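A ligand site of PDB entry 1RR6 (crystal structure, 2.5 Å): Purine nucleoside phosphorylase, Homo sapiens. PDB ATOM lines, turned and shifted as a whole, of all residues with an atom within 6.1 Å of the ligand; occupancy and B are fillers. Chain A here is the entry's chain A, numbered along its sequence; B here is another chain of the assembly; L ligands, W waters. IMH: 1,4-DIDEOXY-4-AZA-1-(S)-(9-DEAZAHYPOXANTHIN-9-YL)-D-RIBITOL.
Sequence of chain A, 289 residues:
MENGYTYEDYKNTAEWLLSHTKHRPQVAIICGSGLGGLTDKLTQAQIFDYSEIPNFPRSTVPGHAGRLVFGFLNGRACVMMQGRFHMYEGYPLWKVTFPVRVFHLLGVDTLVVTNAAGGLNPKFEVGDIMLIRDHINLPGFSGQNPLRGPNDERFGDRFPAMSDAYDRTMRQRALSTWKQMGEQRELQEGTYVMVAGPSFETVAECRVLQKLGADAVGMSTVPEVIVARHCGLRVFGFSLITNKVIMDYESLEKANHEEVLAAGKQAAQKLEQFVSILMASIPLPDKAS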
ATOM      1  N   SER A  33     -10.021  21.006 -15.502  1.00  0.00           N
ATOM      2  CA  SER A  33      -9.281  19.943 -14.828  1.00  0.00           C
ATOM      3  C   SER A  33     -10.123  18.663 -14.638  1.00  0.00           C
ATOM      4  O   SER A  33     -11.245  18.712 -14.143  1.00  0.00           O
ATOM      5  CB  SER A  33      -8.802  20.455 -13.466  1.00  0.00           C
ATOM      6  OG  SER A  33      -8.073  19.463 -12.761  1.00  0.00           O
ATOM      7  N   HIS A  86      -2.684  28.519 -18.030  1.00  0.00           N
ATOM      8  CA  HIS A  86      -3.028  29.364 -16.899  1.00  0.00           C
ATOM      9  C   HIS A  86      -1.985  30.439 -16.655  1.00  0.00           C
ATOM     10  O   HIS A  86      -0.832  30.323 -17.058  1.00  0.00           O
ATOM     11  CB  HIS A  86      -3.160  28.552 -15.601  1.00  0.00           C
ATOM     12  CG  HIS A  86      -3.992  27.328 -15.726  1.00  0.00           C
ATOM     13  ND1 HIS A  86      -3.503  26.156 -16.262  1.00  0.00           N
ATOM     14  CD2 HIS A  86      -5.267  27.075 -15.344  1.00  0.00           C
ATOM     15  CE1 HIS A  86      -4.440  25.222 -16.199  1.00  0.00           C
ATOM     16  NE2 HIS A  86      -5.521  25.754 -15.650  1.00  0.00           N
ATOM     17  N   TYR A  88      -0.904  31.343 -13.668  1.00  0.00           N
ATOM     18  CA  TYR A  88       0.049  30.891 -12.647  1.00  0.00           C
ATOM     19  C   TYR A  88       1.245  30.126 -13.229  1.00  0.00           C
ATOM     20  O   TYR A  88       2.264  29.980 -12.548  1.00  0.00           O
ATOM     21  CB  TYR A  88      -0.650  30.069 -11.554  1.00  0.00           C
ATOM     22  CG  TYR A  88      -1.305  28.788 -12.019  1.00  0.00           C
ATOM     23  CD1 TYR A  88      -0.560  27.669 -12.376  1.00  0.00           C
ATOM     24  CD2 TYR A  88      -2.700  28.696 -12.093  1.00  0.00           C
ATOM     25  CE1 TYR A  88      -1.182  26.489 -12.805  1.00  0.00           C
ATOM     26  CE2 TYR A  88      -3.316  27.527 -12.515  1.00  0.00           C
ATOM     27  CZ  TYR A  88      -2.565  26.428 -12.865  1.00  0.00           C
ATOM     28  OH  TYR A  88      -3.202  25.279 -13.283  1.00  0.00           O
ATOM     29  N   ALA A 116     -12.657  23.302 -12.699  1.00  0.00           N
ATOM     30  CA  ALA A 116     -12.792  22.762 -11.357  1.00  0.00           C
ATOM     31  C   ALA A 116     -12.678  23.971 -10.442  1.00  0.00           C
ATOM     32  O   ALA A 116     -11.905  24.876 -10.745  1.00  0.00           O
ATOM     33  CB  ALA A 116     -11.655  21.785 -11.073  1.00  0.00           C
ATOM     34  N   ALA A 117     -13.433  24.010  -9.346  1.00  0.00           N
ATOM     35  CA  ALA A 117     -13.374  25.159  -8.449  1.00  0.00           C
ATOM     36  C   ALA A 117     -13.802  24.848  -7.026  1.00  0.00           C
ATOM     37  O   ALA A 117     -14.472  23.849  -6.763  1.00  0.00           O
ATOM     38  CB  ALA A 117     -14.214  26.290  -8.996  1.00  0.00           C
ATOM     39  N   GLY A 118     -13.394  25.712  -6.102  1.00  0.00           N
ATOM     40  CA  GLY A 118     -13.738  25.518  -4.709  1.00  0.00           C
ATOM     41  C   GLY A 118     -15.133  26.042  -4.448  1.00  0.00           C
ATOM     42  O   GLY A 118     -15.675  26.827  -5.241  1.00  0.00           O
ATOM     43  N   GLY A 119     -15.723  25.629  -3.339  1.00  0.00           N
ATOM     44  CA  GLY A 119     -17.061  26.074  -3.017  1.00  0.00           C
ATOM     45  C   GLY A 119     -17.087  27.161  -1.964  1.00  0.00           C
ATOM     46  O   GLY A 119     -16.674  26.964  -0.820  1.00  0.00           O
ATOM     47  N   TYR A 192     -18.740  33.022 -10.554  1.00  0.00           N
ATOM     48  CA  TYR A 192     -17.402  32.441 -10.528  1.00  0.00           C
ATOM     49  C   TYR A 192     -16.360  33.544 -10.336  1.00  0.00           C
ATOM     50  O   TYR A 192     -16.278  34.468 -11.153  1.00  0.00           O
ATOM     51  CB  TYR A 192     -17.120  31.719 -11.844  1.00  0.00           C
ATOM     52  CG  TYR A 192     -15.714  31.191 -11.962  1.00  0.00           C
ATOM     53  CD1 TYR A 192     -15.394  29.925 -11.487  1.00  0.00           C
ATOM     54  CD2 TYR A 192     -14.701  31.960 -12.550  1.00  0.00           C
ATOM     55  CE1 TYR A 192     -14.102  29.429 -11.606  1.00  0.00           C
ATOM     56  CE2 TYR A 192     -13.409  31.464 -12.668  1.00  0.00           C
ATOM     57  CZ  TYR A 192     -13.124  30.199 -12.191  1.00  0.00           C
ATOM     58  OH  TYR A 192     -11.872  29.652 -12.341  1.00  0.00           O
ATOM     59  N   VAL A 195      -9.009  34.088  -9.410  1.00  0.00           N
ATOM     60  CA  VAL A 195      -7.827  34.532  -8.672  1.00  0.00           C
ATOM     61  C   VAL A 195      -6.699  33.898  -9.496  1.00  0.00           C
ATOM     62  O   VAL A 195      -6.945  32.938 -10.238  1.00  0.00           O
ATOM     63  CB  VAL A 195      -7.789  34.004  -7.224  1.00  0.00           C
ATOM     64  CG1 VAL A 195      -8.941  34.576  -6.443  1.00  0.00           C
ATOM     65  CG2 VAL A 195      -7.842  32.493  -7.212  1.00  0.00           C
ATOM     66  N   SER A 199      -1.205  29.166  -5.327  1.00  0.00           N
ATOM     67  CA  SER A 199      -1.408  28.709  -3.948  1.00  0.00           C
ATOM     68  C   SER A 199      -2.888  28.857  -3.609  1.00  0.00           C
ATOM     69  O   SER A 199      -3.585  29.652  -4.244  1.00  0.00           O
ATOM     70  CB  SER A 199      -0.536  29.528  -2.980  1.00  0.00           C
ATOM     71  OG  SER A 199      -1.043  30.838  -2.738  1.00  0.00           O
ATOM     72  N   PHE A 200      -3.381  28.107  -2.615  1.00  0.00           N
ATOM     73  CA  PHE A 200      -4.797  28.157  -2.221  1.00  0.00           C
ATOM     74  C   PHE A 200      -5.144  29.257  -1.222  1.00  0.00           C
ATOM     75  O   PHE A 200      -4.299  29.737  -0.463  1.00  0.00           O
ATOM     76  CB  PHE A 200      -5.258  26.787  -1.666  1.00  0.00           C
ATOM     77  CG  PHE A 200      -5.486  25.713  -2.736  1.00  0.00           C
ATOM     78  CD1 PHE A 200      -6.280  25.957  -3.850  1.00  0.00           C
ATOM     79  CD2 PHE A 200      -4.942  24.430  -2.576  1.00  0.00           C
ATOM     80  CE1 PHE A 200      -6.543  24.949  -4.807  1.00  0.00           C
ATOM     81  CE2 PHE A 200      -5.194  23.402  -3.516  1.00  0.00           C
ATOM     82  CZ  PHE A 200      -5.993  23.666  -4.638  1.00  0.00           C
ATOM     83  N   GLU A 201      -6.408  29.647  -1.223  1.00  0.00           N
ATOM     84  CA  GLU A 201      -6.894  30.713  -0.369  1.00  0.00           C
ATOM     85  C   GLU A 201      -6.722  30.424   1.106  1.00  0.00           C
ATOM     86  O   GLU A 201      -6.849  29.273   1.521  1.00  0.00           O
ATOM     87  CB  GLU A 201      -8.383  30.975  -0.634  1.00  0.00           C
ATOM     88  CG  GLU A 201      -8.761  31.421  -2.042  1.00  0.00           C
ATOM     89  CD  GLU A 201      -8.603  30.322  -3.071  1.00  0.00           C
ATOM     90  OE1 GLU A 201      -8.997  29.169  -2.803  1.00  0.00           O
ATOM     91  OE2 GLU A 201      -8.087  30.617  -4.169  1.00  0.00           O
ATOM     92  N   VAL A 217     -14.668  29.560  -6.711  1.00  0.00           N
ATOM     93  CA  VAL A 217     -13.386  30.165  -7.059  1.00  0.00           C
ATOM     94  C   VAL A 217     -12.441  29.257  -7.807  1.00  0.00           C
ATOM     95  O   VAL A 217     -12.201  28.118  -7.427  1.00  0.00           O
ATOM     96  CB  VAL A 217     -12.647  30.659  -5.785  1.00  0.00           C
ATOM     97  CG1 VAL A 217     -12.339  29.483  -4.860  1.00  0.00           C
ATOM     98  CG2 VAL A 217     -11.364  31.372  -6.188  1.00  0.00           C
ATOM     99  N   GLY A 218     -11.889  29.782  -8.890  1.00  0.00           N
ATOM    100  CA  GLY A 218     -10.949  29.031  -9.704  1.00  0.00           C
ATOM    101  C   GLY A 218      -9.847  29.943 -10.188  1.00  0.00           C
ATOM    102  O   GLY A 218      -9.835  31.137  -9.891  1.00  0.00           O
ATOM    103  N   MET A 219      -8.917  29.395 -10.961  1.00  0.00           N
ATOM    104  CA  MET A 219      -7.801  30.167 -11.451  1.00  0.00           C
ATOM    105  C   MET A 219      -7.734  30.179 -12.977  1.00  0.00           C
ATOM    106  O   MET A 219      -6.653  30.158 -13.542  1.00  0.00           O
ATOM    107  CB  MET A 219      -6.511  29.581 -10.867  1.00  0.00           C
ATOM    108  CG  MET A 219      -6.707  29.116  -9.430  1.00  0.00           C
ATOM    109  SD  MET A 219      -5.254  28.563  -8.492  1.00  0.00           S
ATOM    110  CE  MET A 219      -4.423  27.679  -9.648  1.00  0.00           C
ATOM    111  N   SER A 220      -8.886  30.240 -13.627  1.00  0.00           N
ATOM    112  CA  SER A 220      -8.927  30.227 -15.094  1.00  0.00           C
ATOM    113  C   SER A 220     -10.249  30.754 -15.650  1.00  0.00           C
ATOM    114  O   SER A 220     -10.964  31.515 -14.988  1.00  0.00           O
ATOM    115  CB  SER A 220      -8.771  28.793 -15.552  1.00  0.00           C
ATOM    116  OG  SER A 220      -9.812  28.003 -14.980  1.00  0.00           O
ATOM    117  N   THR A 242     -15.217  20.787  -6.758  1.00  0.00           N
ATOM    118  CA  THR A 242     -14.374  19.683  -6.291  1.00  0.00           C
ATOM    119  C   THR A 242     -14.051  19.722  -4.806  1.00  0.00           C
ATOM    120  O   THR A 242     -13.574  18.738  -4.246  1.00  0.00           O
ATOM    121  CB  THR A 242     -13.057  19.660  -7.042  1.00  0.00           C
ATOM    122  OG1 THR A 242     -12.370  20.899  -6.842  1.00  0.00           O
ATOM    123  CG2 THR A 242     -13.275  19.428  -8.527  1.00  0.00           C
ATOM    124  N   ASN A 243     -14.304  20.855  -4.161  1.00  0.00           N
ATOM    125  CA  ASN A 243     -14.006  20.972  -2.746  1.00  0.00           C
ATOM    126  C   ASN A 243     -14.628  22.229  -2.159  1.00  0.00           C
ATOM    127  O   ASN A 243     -14.858  23.202  -2.873  1.00  0.00           O
ATOM    128  CB  ASN A 243     -12.479  21.037  -2.533  1.00  0.00           C
ATOM    129  CG  ASN A 243     -11.838  22.238  -3.236  1.00  0.00           C
ATOM    130  OD1 ASN A 243     -11.771  22.303  -4.472  1.00  0.00           O
ATOM    131  ND2 ASN A 243     -11.376  23.206  -2.446  1.00  0.00           N
ATOM    132  N   VAL A 245     -14.205  25.351   0.283  1.00  0.00           N
ATOM    133  CA  VAL A 245     -13.058  26.087   0.811  1.00  0.00           C
ATOM    134  C   VAL A 245     -13.152  26.164   2.329  1.00  0.00           C
ATOM    135  O   VAL A 245     -14.237  26.285   2.882  1.00  0.00           O
ATOM    136  CB  VAL A 245     -12.990  27.521   0.205  1.00  0.00           C
ATOM    137  CG1 VAL A 245     -13.018  27.436  -1.306  1.00  0.00           C
ATOM    138  CG2 VAL A 245     -14.126  28.382   0.712  1.00  0.00           C
ATOM    139  N   ALA A 255      -6.802  22.121   1.451  1.00  0.00           N
ATOM    140  CA  ALA A 255      -7.139  21.886   0.058  1.00  0.00           C
ATOM    141  C   ALA A 255      -5.889  21.345  -0.648  1.00  0.00           C
ATOM    142  O   ALA A 255      -4.772  21.770  -0.366  1.00  0.00           O
ATOM    143  CB  ALA A 255      -7.580  23.196  -0.590  1.00  0.00           C
ATOM    144  N   ASN A 256      -6.080  20.388  -1.548  1.00  0.00           N
ATOM    145  CA  ASN A 256      -4.953  19.799  -2.246  1.00  0.00           C
ATOM    146  C   ASN A 256      -5.355  19.256  -3.604  1.00  0.00           C
ATOM    147  O   ASN A 256      -6.500  18.874  -3.827  1.00  0.00           O
ATOM    148  CB  ASN A 256      -4.329  18.695  -1.392  1.00  0.00           C
ATOM    149  CG  ASN A 256      -5.371  17.768  -0.765  1.00  0.00           C
ATOM    150  OD1 ASN A 256      -6.061  17.037  -1.472  1.00  0.00           O
ATOM    151  ND2 ASN A 256      -5.490  17.817   0.559  1.00  0.00           N
ATOM    152  N   HIS A 257      -4.388  19.232  -4.512  1.00  0.00           N
ATOM    153  CA  HIS A 257      -4.604  18.766  -5.865  1.00  0.00           C
ATOM    154  C   HIS A 257      -5.131  17.322  -5.878  1.00  0.00           C
ATOM    155  O   HIS A 257      -5.773  16.890  -6.836  1.00  0.00           O
ATOM    156  CB  HIS A 257      -3.296  18.851  -6.650  1.00  0.00           C
ATOM    157  CG  HIS A 257      -3.463  18.810  -8.130  1.00  0.00           C
ATOM    158  ND1 HIS A 257      -4.383  19.586  -8.806  1.00  0.00           N
ATOM    159  CD2 HIS A 257      -2.791  18.117  -9.079  1.00  0.00           C
ATOM    160  CE1 HIS A 257      -4.262  19.388 -10.101  1.00  0.00           C
ATOM    161  NE2 HIS A 257      -3.306  18.503 -10.300  1.00  0.00           N
ATOM    162  N   VAL A 260      -8.878  17.449  -5.238  1.00  0.00           N
ATOM    163  CA  VAL A 260      -9.487  18.058  -6.431  1.00  0.00           C
ATOM    164  C   VAL A 260      -9.550  17.096  -7.622  1.00  0.00           C
ATOM    165  O   VAL A 260     -10.590  16.975  -8.265  1.00  0.00           O
ATOM    166  CB  VAL A 260      -8.725  19.349  -6.839  1.00  0.00           C
ATOM    167  CG1 VAL A 260      -9.419  20.010  -8.030  1.00  0.00           C
ATOM    168  CG2 VAL A 260      -8.660  20.300  -5.661  1.00  0.00           C
ATOM    169  N   LEU A 261      -8.444  16.415  -7.919  1.00  0.00           N
ATOM    170  CA  LEU A 261      -8.410  15.465  -9.034  1.00  0.00           C
ATOM    171  C   LEU A 261      -9.291  14.240  -8.752  1.00  0.00           C
ATOM    172  O   LEU A 261      -9.823  13.627  -9.688  1.00  0.00           O
ATOM    173  CB  LEU A 261      -6.978  15.001  -9.301  1.00  0.00           C
ATOM    174  CG  LEU A 261      -5.963  16.046  -9.759  1.00  0.00           C
ATOM    175  CD1 LEU A 261      -4.587  15.390  -9.824  1.00  0.00           C
ATOM    176  CD2 LEU A 261      -6.354  16.614 -11.109  1.00  0.00           C
ATOM    177  N   PHE B 159       0.213  23.499  -6.223  1.00  0.00           N
ATOM    178  CA  PHE B 159      -0.866  24.206  -5.553  1.00  0.00           C
ATOM    179  C   PHE B 159      -0.792  24.021  -4.031  1.00  0.00           C
ATOM    180  O   PHE B 159      -1.562  23.247  -3.456  1.00  0.00           O
ATOM    181  CB  PHE B 159      -2.223  23.666  -6.037  1.00  0.00           C
ATOM    182  CG  PHE B 159      -2.395  23.643  -7.541  1.00  0.00           C
ATOM    183  CD1 PHE B 159      -2.657  24.818  -8.261  1.00  0.00           C
ATOM    184  CD2 PHE B 159      -2.308  22.441  -8.231  1.00  0.00           C
ATOM    185  CE1 PHE B 159      -2.842  24.780  -9.651  1.00  0.00           C
ATOM    186  CE2 PHE B 159      -2.486  22.393  -9.627  1.00  0.00           C
ATOM    187  CZ  PHE B 159      -2.756  23.568 -10.341  1.00  0.00           C
HETATM  188  O5' IMH L   1      -6.248  21.717  -8.582  1.00  0.00           O
HETATM  189  C5' IMH L   1      -5.888  23.049  -8.905  1.00  0.00           C
HETATM  190  C4' IMH L   1      -6.694  23.471 -10.078  1.00  0.00           C
HETATM  191  N4' IMH L   1      -8.114  23.415  -9.829  1.00  0.00           N
HETATM  192  C3' IMH L   1      -6.360  24.881 -10.472  1.00  0.00           C
HETATM  193  O3' IMH L   1      -6.094  24.825 -11.884  1.00  0.00           O
HETATM  194  C2' IMH L   1      -7.584  25.676 -10.123  1.00  0.00           C
HETATM  195  O2' IMH L   1      -7.948  26.566 -11.199  1.00  0.00           O
HETATM  196  C1' IMH L   1      -8.767  24.707  -9.804  1.00  0.00           C
HETATM  197  C9  IMH L   1      -9.312  24.888  -8.367  1.00  0.00           C
HETATM  198  C8  IMH L   1     -10.067  23.938  -7.696  1.00  0.00           C
HETATM  199  N7  IMH L   1     -10.420  24.277  -6.478  1.00  0.00           N
HETATM  200  C5  IMH L   1      -9.889  25.539  -6.285  1.00  0.00           C
HETATM  201  C6  IMH L   1      -9.952  26.411  -5.120  1.00  0.00           C
HETATM  202  O6  IMH L   1     -10.514  26.176  -4.051  1.00  0.00           O
HETATM  203  N1  IMH L   1      -9.277  27.634  -5.292  1.00  0.00           N
HETATM  204  C2  IMH L   1      -8.609  28.013  -6.461  1.00  0.00           C
HETATM  205  N3  IMH L   1      -8.532  27.183  -7.562  1.00  0.00           N
HETATM  206  C4  IMH L   1      -9.196  25.959  -7.424  1.00  0.00           C
HETATM  207  O   HOH W   1      -9.712  26.697  -1.659  1.00  0.00           O
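O of Ala 117 lies within hydrogen-bond range of N of Thr 242. The backbone NH (N) of Met 219 lies within hydrogen-bond range of the side-chain hydroxyl (OH) of Tyr 192. The backbone NH (N) of Val 245 is in hydrogen-bond range of the backbone carbonyl oxygen (O) of Gly 119, 3.1 Å away. The backbone carbonyl oxygen of Asn 243 sits at hydrogen-bond distance from the backbone NH of Gly 119. N of Gly 118 sits at hydrogen-bond distance from O of Val 217 (3.0 Å). The backbone NH (N) of Val 195 is in hydrogen-bond range of the backbone carbonyl oxygen (O) of Gly 218 (3.1 Å). ND1 of His 86 is in hydrogen-bond range of OH of Tyr 88 (3.1 Å). The side-chain hydroxyl (OG1) of Thr 242 sits at hydrogen-bond distance from the side-chain amide oxygen (OD1) of Asn 243 (2.8 Å).
A nitrogen (N3) of the ligand lies close to the side-chain sulfur (SD) of Met 219, at 3.7 Å. The side-chain hydroxyl of Tyr 88 lies within hydrogen-bond range of an oxygen (O3') of the ligand, 3.2 Å away. The backbone NH (N) of Gly 118 sits close to a nitrogen (N7) of the ligand (3.3 Å). N7 of the ligand sits at hydrogen-bond distance from OD1 of Asn 243 (3.1 Å). A nitrogen (N1) of the ligand lies within hydrogen-bond range of the side-chain carboxylate of Glu 201, 2.9 Å away. A ring nitrogen (ND1) of His 257 sits at hydrogen-bond distance from an oxygen (O5') of the ligand, at 2.8 Å. N of Met 219 is in hydrogen-bond range of O2' of the ligand, at 3.0 Å.
Water W1 bridges an oxygen (O6) of the ligand (2.6 Å) and the side-chain carboxylate of Glu 201 (2.8 Å).
His 86 touches the ligand (NE2 to O3', 3.9 Å). O of Ala 116 touches C1' of the ligand (3.3 Å). Ala 117 touches the ligand (C to N7, 3.5 Å). CE1 of Phe 200 touches C5 of the ligand, 3.7 Å away. Val 217 touches the ligand. Gly 218 touches the ligand. Thr 242 touches the ligand (OG1 to C8, 3.9 Å). CG1 of Val 245 touches O6 of the ligand, at 3.9 Å. Val 260 touches the ligand. CZ of Phe 159 of chain B touches C5' of the ligand (3.5 Å). Hydrophobic or aromatic side chains within 4 Å of the ligand: Tyr 88, Phe 200, Val 217, Met 219, Val 245, His 257, Val 260 and Phe 159 of chain B. Of the 25 residues printed, 16 come within 4 Å of the ligand.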
